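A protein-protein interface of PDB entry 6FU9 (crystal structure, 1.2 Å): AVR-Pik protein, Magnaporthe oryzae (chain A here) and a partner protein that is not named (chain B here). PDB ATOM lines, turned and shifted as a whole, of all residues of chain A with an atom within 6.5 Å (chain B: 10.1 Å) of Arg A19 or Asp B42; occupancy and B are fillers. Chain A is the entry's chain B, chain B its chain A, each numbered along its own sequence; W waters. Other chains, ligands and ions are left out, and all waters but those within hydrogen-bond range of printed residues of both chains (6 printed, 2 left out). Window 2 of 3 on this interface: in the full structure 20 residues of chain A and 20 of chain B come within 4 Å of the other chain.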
ATOM      1  N   ARG A  11     -29.237   6.585  -8.626  1.00  0.00           N
ATOM      2  CA  ARG A  11     -28.012   7.177  -9.204  1.00  0.00           C
ATOM      3  C   ARG A  11     -27.687   6.583 -10.563  1.00  0.00           C
ATOM      4  O   ARG A  11     -28.030   5.420 -10.851  1.00  0.00           O
ATOM      5  CB  ARG A  11     -26.775   7.015  -8.257  1.00  0.00           C
ATOM      6  CG  ARG A  11     -26.217   5.608  -8.116  1.00  0.00           C
ATOM      7  CD  ARG A  11     -25.001   5.511  -7.195  1.00  0.00           C
ATOM      8  NE  ARG A  11     -24.606   4.117  -7.027  1.00  0.00           N
ATOM      9  CZ  ARG A  11     -24.431   3.465  -5.857  1.00  0.00           C
ATOM     10  NH1 ARG A  11     -24.648   4.029  -4.670  1.00  0.00           N
ATOM     11  NH2 ARG A  11     -24.092   2.203  -5.885  1.00  0.00           N
ATOM     12  N   LEU A  15     -19.500   2.394 -10.698  1.00  0.00           N
ATOM     13  CA  LEU A  15     -18.881   1.235 -10.103  1.00  0.00           C
ATOM     14  C   LEU A  15     -18.047   1.555  -8.876  1.00  0.00           C
ATOM     15  O   LEU A  15     -17.812   0.659  -8.068  1.00  0.00           O
ATOM     16  CB  LEU A  15     -18.002   0.444 -11.056  1.00  0.00           C
ATOM     17  CG  LEU A  15     -18.745  -0.162 -12.262  1.00  0.00           C
ATOM     18  CD1 LEU A  15     -17.787  -1.132 -12.947  1.00  0.00           C
ATOM     19  CD2 LEU A  15     -20.028  -0.903 -11.866  1.00  0.00           C
ATOM     20  N   ARG A  17     -19.091   3.182  -6.416  1.00  0.00           N
ATOM     21  CA  ARG A  17     -19.977   3.114  -5.262  1.00  0.00           C
ATOM     22  C   ARG A  17     -20.634   1.781  -5.091  1.00  0.00           C
ATOM     23  O   ARG A  17     -21.389   1.601  -4.125  1.00  0.00           O
ATOM     24  CB  ARG A  17     -20.975   4.221  -5.303  1.00  0.00           C
ATOM     25  CG  ARG A  17     -20.196   5.543  -5.280  1.00  0.00           C
ATOM     26  CD  ARG A  17     -21.055   6.731  -5.049  1.00  0.00           C
ATOM     27  NE  ARG A  17     -21.880   6.592  -3.842  1.00  0.00           N
ATOM     28  CZ  ARG A  17     -23.086   7.141  -3.701  1.00  0.00           C
ATOM     29  NH1 ARG A  17     -23.628   7.873  -4.697  1.00  0.00           N
ATOM     30  NH2 ARG A  17     -23.760   6.876  -2.642  1.00  0.00           N
ATOM     31  N   GLU A  18     -20.365   0.837  -6.014  1.00  0.00           N
ATOM     32  CA  GLU A  18     -21.022  -0.489  -5.896  1.00  0.00           C
ATOM     33  C   GLU A  18     -20.331  -1.366  -4.862  1.00  0.00           C
ATOM     34  O   GLU A  18     -19.087  -1.463  -4.872  1.00  0.00           O
ATOM     35  CB  GLU A  18     -20.992  -1.162  -7.257  1.00  0.00           C
ATOM     36  CG  GLU A  18     -21.994  -0.563  -8.223  1.00  0.00           C
ATOM     37  CD  GLU A  18     -23.438  -0.675  -7.776  1.00  0.00           C
ATOM     38  OE1 GLU A  18     -23.805  -1.633  -7.029  1.00  0.00           O
ATOM     39  OE2 GLU A  18     -24.231   0.228  -8.132  1.00  0.00           O
ATOM     40  N   ARG A  19     -21.111  -2.060  -4.017  1.00  0.00           N
ATOM     41  CA  ARG A  19     -20.527  -3.084  -3.160  1.00  0.00           C
ATOM     42  C   ARG A  19     -19.936  -4.173  -4.047  1.00  0.00           C
ATOM     43  O   ARG A  19     -20.409  -4.410  -5.193  1.00  0.00           O
ATOM     44  CB  ARG A  19     -21.543  -3.666  -2.211  1.00  0.00           C
ATOM     45  CG  ARG A  19     -22.617  -4.537  -2.881  1.00  0.00           C
ATOM     46  CD  ARG A  19     -23.768  -4.773  -1.939  1.00  0.00           C
ATOM     47  NE  ARG A  19     -24.806  -5.649  -2.465  1.00  0.00           N
ATOM     48  CZ  ARG A  19     -25.807  -5.245  -3.206  1.00  0.00           C
ATOM     49  NH1 ARG A  19     -25.814  -4.052  -3.777  1.00  0.00           N
ATOM     50  NH2 ARG A  19     -26.779  -6.098  -3.475  1.00  0.00           N
ATOM     51  N   ASP A  20     -18.914  -4.872  -3.543  1.00  0.00           N
ATOM     52  CA  ASP A  20     -18.357  -5.983  -4.316  1.00  0.00           C
ATOM     53  C   ASP A  20     -19.417  -7.008  -4.537  1.00  0.00           C
ATOM     54  O   ASP A  20     -20.405  -7.159  -3.839  1.00  0.00           O
ATOM     55  CB  ASP A  20     -17.151  -6.615  -3.572  1.00  0.00           C
ATOM     56  CG  ASP A  20     -15.881  -5.790  -3.579  1.00  0.00           C
ATOM     57  OD1 ASP A  20     -15.751  -4.764  -4.271  1.00  0.00           O
ATOM     58  OD2 ASP A  20     -14.943  -6.195  -2.837  1.00  0.00           O
ATOM     59  N   PRO A  21     -19.216  -7.836  -5.594  1.00  0.00           N
ATOM     60  CA  PRO A  21     -20.009  -9.046  -5.758  1.00  0.00           C
ATOM     61  C   PRO A  21     -19.863  -9.928  -4.517  1.00  0.00           C
ATOM     62  O   PRO A  21     -18.848  -9.868  -3.808  1.00  0.00           O
ATOM     63  CB  PRO A  21     -19.349  -9.722  -6.999  1.00  0.00           C
ATOM     64  CG  PRO A  21     -18.701  -8.608  -7.707  1.00  0.00           C
ATOM     65  CD  PRO A  21     -18.145  -7.739  -6.623  1.00  0.00           C
ATOM     66  N   ASN A  22     -20.834 -10.803  -4.321  1.00  0.00           N
ATOM     67  CA  ASN A  22     -20.795 -11.843  -3.310  1.00  0.00           C
ATOM     68  C   ASN A  22     -20.296 -13.076  -3.972  1.00  0.00           C
ATOM     69  O   ASN A  22     -21.016 -13.647  -4.780  1.00  0.00           O
ATOM     70  CB  ASN A  22     -22.188 -12.129  -2.750  1.00  0.00           C
ATOM     71  CG  ASN A  22     -22.185 -13.262  -1.775  1.00  0.00           C
ATOM     72  OD1 ASN A  22     -21.328 -13.337  -0.929  1.00  0.00           O
ATOM     73  ND2 ASN A  22     -23.162 -14.123  -1.878  1.00  0.00           N
ATOM     74  N   PHE A  37     -20.792  -6.701 -13.125  1.00  0.00           N
ATOM     75  CA  PHE A  37     -22.026  -6.165 -12.521  1.00  0.00           C
ATOM     76  C   PHE A  37     -23.057  -6.002 -13.655  1.00  0.00           C
ATOM     77  O   PHE A  37     -22.749  -5.410 -14.698  1.00  0.00           O
ATOM     78  CB  PHE A  37     -21.765  -4.766 -11.918  1.00  0.00           C
ATOM     79  CG  PHE A  37     -20.678  -4.729 -10.906  1.00  0.00           C
ATOM     80  CD1 PHE A  37     -19.366  -4.629 -11.309  1.00  0.00           C
ATOM     81  CD2 PHE A  37     -20.951  -4.793  -9.535  1.00  0.00           C
ATOM     82  CE1 PHE A  37     -18.359  -4.605 -10.367  1.00  0.00           C
ATOM     83  CE2 PHE A  37     -19.955  -4.748  -8.614  1.00  0.00           C
ATOM     84  CZ  PHE A  37     -18.667  -4.679  -8.998  1.00  0.00           C
ATOM     85  N   ARG A  44     -29.030  -2.395 -10.320  1.00  0.00           N
ATOM     86  CA  ARG A  44     -28.201  -3.590 -10.191  1.00  0.00           C
ATOM     87  C   ARG A  44     -29.058  -4.830 -10.070  1.00  0.00           C
ATOM     88  O   ARG A  44     -29.976  -4.876  -9.232  1.00  0.00           O
ATOM     89  CB  ARG A  44     -27.282  -3.480  -8.986  1.00  0.00           C
ATOM     90  CG  ARG A  44     -26.438  -4.698  -8.713  1.00  0.00           C
ATOM     91  CD  ARG A  44     -25.460  -4.415  -7.616  1.00  0.00           C
ATOM     92  NE  ARG A  44     -24.711  -5.529  -7.162  1.00  0.00           N
ATOM     93  CZ  ARG A  44     -23.553  -5.402  -6.506  1.00  0.00           C
ATOM     94  NH1 ARG A  44     -22.903  -4.236  -6.478  1.00  0.00           N
ATOM     95  NH2 ARG A  44     -23.005  -6.448  -5.978  1.00  0.00           N
ATOM     96  N   GLN A  45     -28.819  -5.818 -10.935  1.00  0.00           N
ATOM     97  CA  GLN A  45     -29.519  -7.072 -10.918  1.00  0.00           C
ATOM     98  C   GLN A  45     -28.715  -8.135 -10.172  1.00  0.00           C
ATOM     99  O   GLN A  45     -29.286  -8.898  -9.364  1.00  0.00           O
ATOM    100  CB  GLN A  45     -29.846  -7.518 -12.337  1.00  0.00           C
ATOM    101  CG  GLN A  45     -30.674  -6.482 -13.131  1.00  0.00           C
ATOM    102  CD  GLN A  45     -32.033  -6.229 -12.535  1.00  0.00           C
ATOM    103  OE1 GLN A  45     -32.858  -7.138 -12.466  1.00  0.00           O
ATOM    104  NE2 GLN A  45     -32.268  -5.020 -12.071  1.00  0.00           N
ATOM    105  N   ASP A  46     -27.432  -8.281 -10.516  1.00  0.00           N
ATOM    106  CA  ASP A  46     -26.572  -9.190  -9.822  1.00  0.00           C
ATOM    107  C   ASP A  46     -25.145  -8.858 -10.233  1.00  0.00           C
ATOM    108  O   ASP A  46     -24.909  -7.885 -10.996  1.00  0.00           O
ATOM    109  CB  ASP A  46     -26.908 -10.715 -10.099  1.00  0.00           C
ATOM    110  CG  ASP A  46     -26.569 -11.678  -8.911  1.00  0.00           C
ATOM    111  OD1 ASP A  46     -25.827 -11.257  -8.002  1.00  0.00           O
ATOM    112  OD2 ASP A  46     -27.050 -12.851  -8.895  1.00  0.00           O
ATOM    113  N   ALA A  47     -24.206  -9.609  -9.662  1.00  0.00           N
ATOM    114  CA  ALA A  47     -22.795  -9.374  -9.847  1.00  0.00           C
ATOM    115  C   ALA A  47     -22.045 -10.648  -9.587  1.00  0.00           C
ATOM    116  O   ALA A  47     -22.520 -11.547  -8.873  1.00  0.00           O
ATOM    117  CB  ALA A  47     -22.322  -8.245  -8.895  1.00  0.00           C
ATOM    118  N   GLY A  48     -20.837 -10.762 -10.140  1.00  0.00           N
ATOM    119  CA  GLY A  48     -20.036 -11.971  -9.993  1.00  0.00           C
ATOM    120  C   GLY A  48     -18.593 -11.736 -10.321  1.00  0.00           C
ATOM    121  O   GLY A  48     -18.118 -10.611 -10.381  1.00  0.00           O
ATOM    122  N   LYS A  88     -14.740  -4.692 -13.885  1.00  0.00           N
ATOM    123  CA  LYS A  88     -13.604  -3.971 -13.337  1.00  0.00           C
ATOM    124  C   LYS A  88     -12.640  -4.931 -12.686  1.00  0.00           C
ATOM    125  O   LYS A  88     -13.015  -6.014 -12.282  1.00  0.00           O
ATOM    126  CB  LYS A  88     -13.922  -2.826 -12.453  1.00  0.00           C
ATOM    127  CG  LYS A  88     -14.551  -3.336 -11.220  1.00  0.00           C
ATOM    128  CD  LYS A  88     -14.685  -2.182 -10.132  1.00  0.00           C
ATOM    129  CE  LYS A  88     -15.401  -2.636  -8.884  1.00  0.00           C
ATOM    130  NZ  LYS A  88     -15.525  -1.662  -7.803  1.00  0.00           N
ATOM    131  N   VAL B  10     -23.120 -21.575 -14.186  1.00  0.00           N
ATOM    132  CA  VAL B  10     -23.824 -20.826 -13.123  1.00  0.00           C
ATOM    133  C   VAL B  10     -25.301 -20.932 -13.356  1.00  0.00           C
ATOM    134  O   VAL B  10     -25.777 -20.634 -14.497  1.00  0.00           O
ATOM    135  CB  VAL B  10     -23.392 -19.368 -13.067  1.00  0.00           C
ATOM    136  CG1 VAL B  10     -24.044 -18.663 -11.832  1.00  0.00           C
ATOM    137  CG2 VAL B  10     -21.889 -19.202 -13.008  1.00  0.00           C
ATOM    138  N   PHE B  11     -26.033 -21.323 -12.311  1.00  0.00           N
ATOM    139  CA  PHE B  11     -27.481 -21.343 -12.313  1.00  0.00           C
ATOM    140  C   PHE B  11     -28.008 -20.212 -11.422  1.00  0.00           C
ATOM    141  O   PHE B  11     -27.341 -19.847 -10.441  1.00  0.00           O
ATOM    142  CB  PHE B  11     -28.042 -22.657 -11.806  1.00  0.00           C
ATOM    143  CG  PHE B  11     -27.643 -23.867 -12.597  1.00  0.00           C
ATOM    144  CD1 PHE B  11     -28.292 -24.163 -13.785  1.00  0.00           C
ATOM    145  CD2 PHE B  11     -26.646 -24.715 -12.187  1.00  0.00           C
ATOM    146  CE1 PHE B  11     -27.958 -25.285 -14.537  1.00  0.00           C
ATOM    147  CE2 PHE B  11     -26.294 -25.826 -12.924  1.00  0.00           C
ATOM    148  CZ  PHE B  11     -26.965 -26.110 -14.096  1.00  0.00           C
ATOM    149  N   LYS B  12     -29.170 -19.694 -11.772  1.00  0.00           N
ATOM    150  CA  LYS B  12     -29.974 -18.851 -10.870  1.00  0.00           C
ATOM    151  C   LYS B  12     -31.128 -19.697 -10.421  1.00  0.00           C
ATOM    152  O   LYS B  12     -31.897 -20.237 -11.227  1.00  0.00           O
ATOM    153  CB  LYS B  12     -30.382 -17.576 -11.589  1.00  0.00           C
ATOM    154  CG  LYS B  12     -29.256 -16.530 -11.692  1.00  0.00           C
ATOM    155  CD  LYS B  12     -28.978 -15.643 -10.447  1.00  0.00           C
ATOM    156  CE  LYS B  12     -29.933 -14.478 -10.391  1.00  0.00           C
ATOM    157  NZ  LYS B  12     -29.793 -13.675  -9.169  1.00  0.00           N
ATOM    158  N   ARG B  21     -30.779 -24.283  -0.183  1.00  0.00           N
ATOM    159  CA  ARG B  21     -29.386 -24.093  -0.545  1.00  0.00           C
ATOM    160  C   ARG B  21     -28.596 -25.363  -0.267  1.00  0.00           C
ATOM    161  O   ARG B  21     -27.825 -25.790  -1.142  1.00  0.00           O
ATOM    162  CB  ARG B  21     -28.748 -22.879   0.157  1.00  0.00           C
ATOM    163  CG  ARG B  21     -29.310 -21.569  -0.343  1.00  0.00           C
ATOM    164  CD  ARG B  21     -28.588 -20.366   0.271  1.00  0.00           C
ATOM    165  NE  ARG B  21     -29.252 -19.158  -0.162  1.00  0.00           N
ATOM    166  CZ  ARG B  21     -30.127 -18.437   0.498  1.00  0.00           C
ATOM    167  NH1 ARG B  21     -30.465 -18.704   1.755  1.00  0.00           N
ATOM    168  NH2 ARG B  21     -30.660 -17.407  -0.128  1.00  0.00           N
ATOM    169  N   ILE B  39     -22.732 -21.314  -3.389  1.00  0.00           N
ATOM    170  CA  ILE B  39     -23.850 -20.421  -3.510  1.00  0.00           C
ATOM    171  C   ILE B  39     -23.302 -19.034  -3.409  1.00  0.00           C
ATOM    172  O   ILE B  39     -22.623 -18.733  -2.449  1.00  0.00           O
ATOM    173  CB  ILE B  39     -24.992 -20.749  -2.490  1.00  0.00           C
ATOM    174  CG1 ILE B  39     -25.642 -22.076  -3.046  1.00  0.00           C
ATOM    175  CG2 ILE B  39     -25.943 -19.576  -2.511  1.00  0.00           C
ATOM    176  CD1 ILE B  39     -26.491 -22.857  -2.126  1.00  0.00           C
ATOM    177  N   ALA B  40     -23.630 -18.186  -4.347  1.00  0.00           N
ATOM    178  CA  ALA B  40     -23.065 -16.832  -4.545  1.00  0.00           C
ATOM    179  C   ALA B  40     -24.206 -15.911  -4.944  1.00  0.00           C
ATOM    180  O   ALA B  40     -25.398 -16.272  -4.870  1.00  0.00           O
ATOM    181  CB  ALA B  40     -21.971 -16.849  -5.628  1.00  0.00           C
ATOM    182  N   GLY B  41     -23.826 -14.712  -5.312  1.00  0.00           N
ATOM    183  CA  GLY B  41     -24.752 -13.727  -5.856  1.00  0.00           C
ATOM    184  C   GLY B  41     -25.326 -12.794  -4.814  1.00  0.00           C
ATOM    185  O   GLY B  41     -25.333 -13.117  -3.593  1.00  0.00           O
ATOM    186  N   ASP B  42     -25.860 -11.696  -5.293  1.00  0.00           N
ATOM    187  CA  ASP B  42     -26.376 -10.701  -4.379  1.00  0.00           C
ATOM    188  C   ASP B  42     -27.483 -11.225  -3.497  1.00  0.00           C
ATOM    189  O   ASP B  42     -27.584 -10.848  -2.318  1.00  0.00           O
ATOM    190  CB  ASP B  42     -26.912  -9.512  -5.150  1.00  0.00           C
ATOM    191  CG  ASP B  42     -25.855  -8.657  -5.826  1.00  0.00           C
ATOM    192  OD1 ASP B  42     -24.652  -8.743  -5.460  1.00  0.00           O
ATOM    193  OD2 ASP B  42     -26.240  -7.841  -6.718  1.00  0.00           O
ATOM    194  N   LEU B  43     -28.332 -12.050  -4.065  1.00  0.00           N
ATOM    195  CA  LEU B  43     -29.476 -12.655  -3.367  1.00  0.00           C
ATOM    196  C   LEU B  43     -29.192 -14.038  -2.847  1.00  0.00           C
ATOM    197  O   LEU B  43     -30.083 -14.756  -2.382  1.00  0.00           O
ATOM    198  CB  LEU B  43     -30.679 -12.621  -4.279  1.00  0.00           C
ATOM    199  CG  LEU B  43     -30.972 -11.239  -4.881  1.00  0.00           C
ATOM    200  CD1 LEU B  43     -32.195 -11.305  -5.786  1.00  0.00           C
ATOM    201  CD2 LEU B  43     -31.167 -10.229  -3.765  1.00  0.00           C
ATOM    202  N   ARG B  44     -27.953 -14.500  -2.984  1.00  0.00           N
ATOM    203  CA  ARG B  44     -27.619 -15.852  -2.476  1.00  0.00           C
ATOM    204  C   ARG B  44     -28.423 -16.888  -3.230  1.00  0.00           C
ATOM    205  O   ARG B  44     -28.864 -17.877  -2.736  1.00  0.00           O
ATOM    206  CB  ARG B  44     -27.639 -16.008  -0.928  1.00  0.00           C
ATOM    207  CG  ARG B  44     -26.439 -15.363  -0.264  1.00  0.00           C
ATOM    208  CD  ARG B  44     -26.333 -13.892  -0.382  1.00  0.00           C
ATOM    209  NE  ARG B  44     -25.292 -13.375   0.511  1.00  0.00           N
ATOM    210  CZ  ARG B  44     -24.771 -12.153   0.451  1.00  0.00           C
ATOM    211  NH1 ARG B  44     -23.845 -11.769   1.321  1.00  0.00           N
ATOM    212  NH2 ARG B  44     -25.174 -11.292  -0.491  1.00  0.00           N
ATOM    213  N   ASP B  45     -28.581 -16.605  -4.537  1.00  0.00           N
ATOM    214  CA  ASP B  45     -29.320 -17.529  -5.378  1.00  0.00           C
ATOM    215  C   ASP B  45     -28.566 -17.918  -6.680  1.00  0.00           C
ATOM    216  O   ASP B  45     -29.168 -18.492  -7.603  1.00  0.00           O
ATOM    217  CB  ASP B  45     -30.704 -17.031  -5.685  1.00  0.00           C
ATOM    218  CG  ASP B  45     -30.761 -15.828  -6.515  1.00  0.00           C
ATOM    219  OD1 ASP B  45     -29.726 -15.321  -6.977  1.00  0.00           O
ATOM    220  OD2 ASP B  45     -31.910 -15.354  -6.748  1.00  0.00           O
ATOM    221  N   GLN B  46     -27.279 -17.612  -6.740  1.00  0.00           N
ATOM    222  CA  GLN B  46     -26.403 -18.096  -7.854  1.00  0.00           C
ATOM    223  C   GLN B  46     -25.761 -19.373  -7.380  1.00  0.00           C
ATOM    224  O   GLN B  46     -25.129 -19.378  -6.317  1.00  0.00           O
ATOM    225  CB  GLN B  46     -25.258 -17.174  -8.116  1.00  0.00           C
ATOM    226  CG  GLN B  46     -25.338 -16.181  -9.157  1.00  0.00           C
ATOM    227  CD  GLN B  46     -24.061 -15.314  -9.255  1.00  0.00           C
ATOM    228  OE1 GLN B  46     -22.912 -15.762  -9.392  1.00  0.00           O
ATOM    229  NE2 GLN B  46     -24.282 -14.065  -9.318  1.00  0.00           N
ATOM    230  N   VAL B  47     -25.877 -20.465  -8.127  1.00  0.00           N
ATOM    231  CA  VAL B  47     -25.211 -21.711  -7.812  1.00  0.00           C
ATOM    232  C   VAL B  47     -24.108 -21.870  -8.834  1.00  0.00           C
ATOM    233  O   VAL B  47     -24.424 -22.007 -10.033  1.00  0.00           O
ATOM    234  CB  VAL B  47     -26.174 -22.872  -7.880  1.00  0.00           C
ATOM    235  CG1 VAL B  47     -25.483 -24.192  -7.607  1.00  0.00           C
ATOM    236  CG2 VAL B  47     -27.348 -22.625  -6.888  1.00  0.00           C
ATOM    237  N   VAL B  48     -22.879 -21.715  -8.417  1.00  0.00           N
ATOM    238  CA  VAL B  48     -21.700 -21.717  -9.277  1.00  0.00           C
ATOM    239  C   VAL B  48     -21.057 -23.087  -9.185  1.00  0.00           C
ATOM    240  O   VAL B  48     -20.634 -23.518  -8.109  1.00  0.00           O
ATOM    241  CB  VAL B  48     -20.710 -20.588  -8.909  1.00  0.00           C
ATOM    242  CG1 VAL B  48     -19.524 -20.658  -9.898  1.00  0.00           C
ATOM    243  CG2 VAL B  48     -21.334 -19.237  -8.867  1.00  0.00           C
ATOM    244  N   LEU B  73     -27.575 -19.192 -16.017  1.00  0.00           N
ATOM    245  CA  LEU B  73     -27.076 -17.830 -16.100  1.00  0.00           C
ATOM    246  C   LEU B  73     -25.827 -17.724 -16.939  1.00  0.00           C
ATOM    247  O   LEU B  73     -25.646 -16.728 -17.640  1.00  0.00           O
ATOM    248  CB  LEU B  73     -26.840 -17.245 -14.657  1.00  0.00           C
ATOM    249  CG  LEU B  73     -26.170 -15.857 -14.570  1.00  0.00           C
ATOM    250  CD1 LEU B  73     -27.012 -14.777 -15.214  1.00  0.00           C
ATOM    251  CD2 LEU B  73     -25.915 -15.501 -13.083  1.00  0.00           C
HETATM  252  O   HOH W   1     -28.893  -7.423  -6.770  1.00  0.00           O
HETATM  253  O   HOH W   2     -24.143  -8.566  -2.600  1.00  0.00           O
HETATM  254  O   HOH W   3     -27.345  -8.177  -1.427  1.00  0.00           O
HETATM  255  O   HOH W   4     -23.185 -16.861  -0.629  1.00  0.00           O
HETATM  256  O   HOH W   5     -31.079 -11.143  -9.688  1.00  0.00           O
HETATM  257  O   HOH W   6     -20.564 -14.486  -7.499  1.00  0.00           O
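Of the printed residues of chain B, Arg A19 touches Asp B42 (3.6 Å).
No residue of chain B comes within 4 Å of Asp A20.
No residue of chain B comes within 4 Å of Pro A21.
Of the printed residues of chain B, Asn A22 touches Ala B40, Gly B41 and Arg B44.
Of the printed residues of chain B, Arg A44 touches Asp B42.
Asp A46 touches four residues of chain B.
Printed residues of chain A within 4 Å of Ala B40: Asn A22.
Of the printed residues of chain A, Asp B42 touches Arg A19 (3.6 Å), Arg A44 (2.8 Å), Asp A46 (2.7 Å) and Ala A47 (3.99 Å).
The nearest printed residue of chain A that does not touch Ala B40 is Asp A46 (5.5 Å).
NE of Arg B21 sits at hydrogen-bond distance from O of Arg B44 (2.9 Å).
The backbone carbonyl oxygen (O) of Ala B40 lies within hydrogen-bond range of the backbone NH (N) of Asp B45 (3.2 Å).
The backbone carbonyl oxygen of Gln B46 lies within hydrogen-bond range of the backbone NH of Ala B40, 2.7 Å away.
The side-chain carboxylate (OE1) of Glu A18 lies within salt-bridge range of the guanidinium group (NH1) of Arg A44 (2.8 Å).
The backbone carbonyl oxygen (O) of Arg A19 lies within hydrogen-bond range of the guanidinium group (NH1) of Arg A44, at 2.8 Å.
NH2 of Arg A44 is in hydrogen-bond range of O of Asp A20 (3.4 Å).
OD2 of Asp A46 is in salt-bridge range of NZ of Lys B12 (2.9 Å).
The backbone carbonyl oxygen (O) of Gly B41 sits at hydrogen-bond distance from the side-chain amide nitrogen (ND2) of Asn A22 (2.9 Å).
OD2 of Asp B42 is in salt-bridge range of NH2 of Arg A19 (3.7 Å).
NE of Arg A44 is in salt-bridge range of OD2 of Asp B42, at 2.8 Å.
The backbone NH (N) of Asp B42 sits at hydrogen-bond distance from the side-chain carboxylate (OD1) of Asp A46, 2.7 Å away.
NE of Arg B44 lies close to ND2 of Asn A22, at 3.3 Å.
The side-chain carboxylate of Asp A46 sits at hydrogen-bond distance from the side-chain amide nitrogen of Gln B46, at 3.1 Å.
The backbone carbonyl oxygen (O) of Ala A47 is in hydrogen-bond range of the side-chain amide nitrogen (NE2) of Gln B46, at 3.1 Å.
Asn A22 touches Ala B40.
OD1 of Asp A46 touches CA of Gly B41 (3.4 Å).
Asp B42 touches Ala A47 (OD2 to N, 3.99 Å).
Water W4 lies within hydrogen-bond range of O of Ile B39 and ND2 of Asn A22.
Water W1 lies within hydrogen-bond range of OD2 of Asp B42 (2.7 Å) and O of Gln A45 (3.0 Å).
Water W3 lies within hydrogen-bond range of O of Asp B42 (2.8 Å) and NH2 of Arg A19 (3.0 Å).
Water W6 lies within hydrogen-bond range of the backbone carbonyl oxygen of Asn A22 (2.9 Å) and the side-chain amide oxygen of Gln B46 (3.3 Å).
Water W5 bridges the side-chain amino group (NZ) of Lys B12 (2.9 Å) and the backbone carbonyl oxygen (O) of Gln A45 (2.9 Å).
Water W2 lies within hydrogen-bond range of the side-chain carboxylate (OD1) of Asp B42 (2.9 Å) and the guanidinium group (NE) of Arg A19 (3.0 Å).
Hydrophobic or aromatic side chains of chain B that line the printed part of chain A: Ala B40.
Among the printed residues, 11 pairs touch across the chains.
Among the printed residues, Asp or Glu carboxylates within 4 Å of a Lys or Arg side-chain nitrogen of the other chain: Arg A19 with Asp B42 (3.7 Å), Arg A44 with Asp B42 (2.8 Å) and Asp A46 with Lys B12 (2.9 Å).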
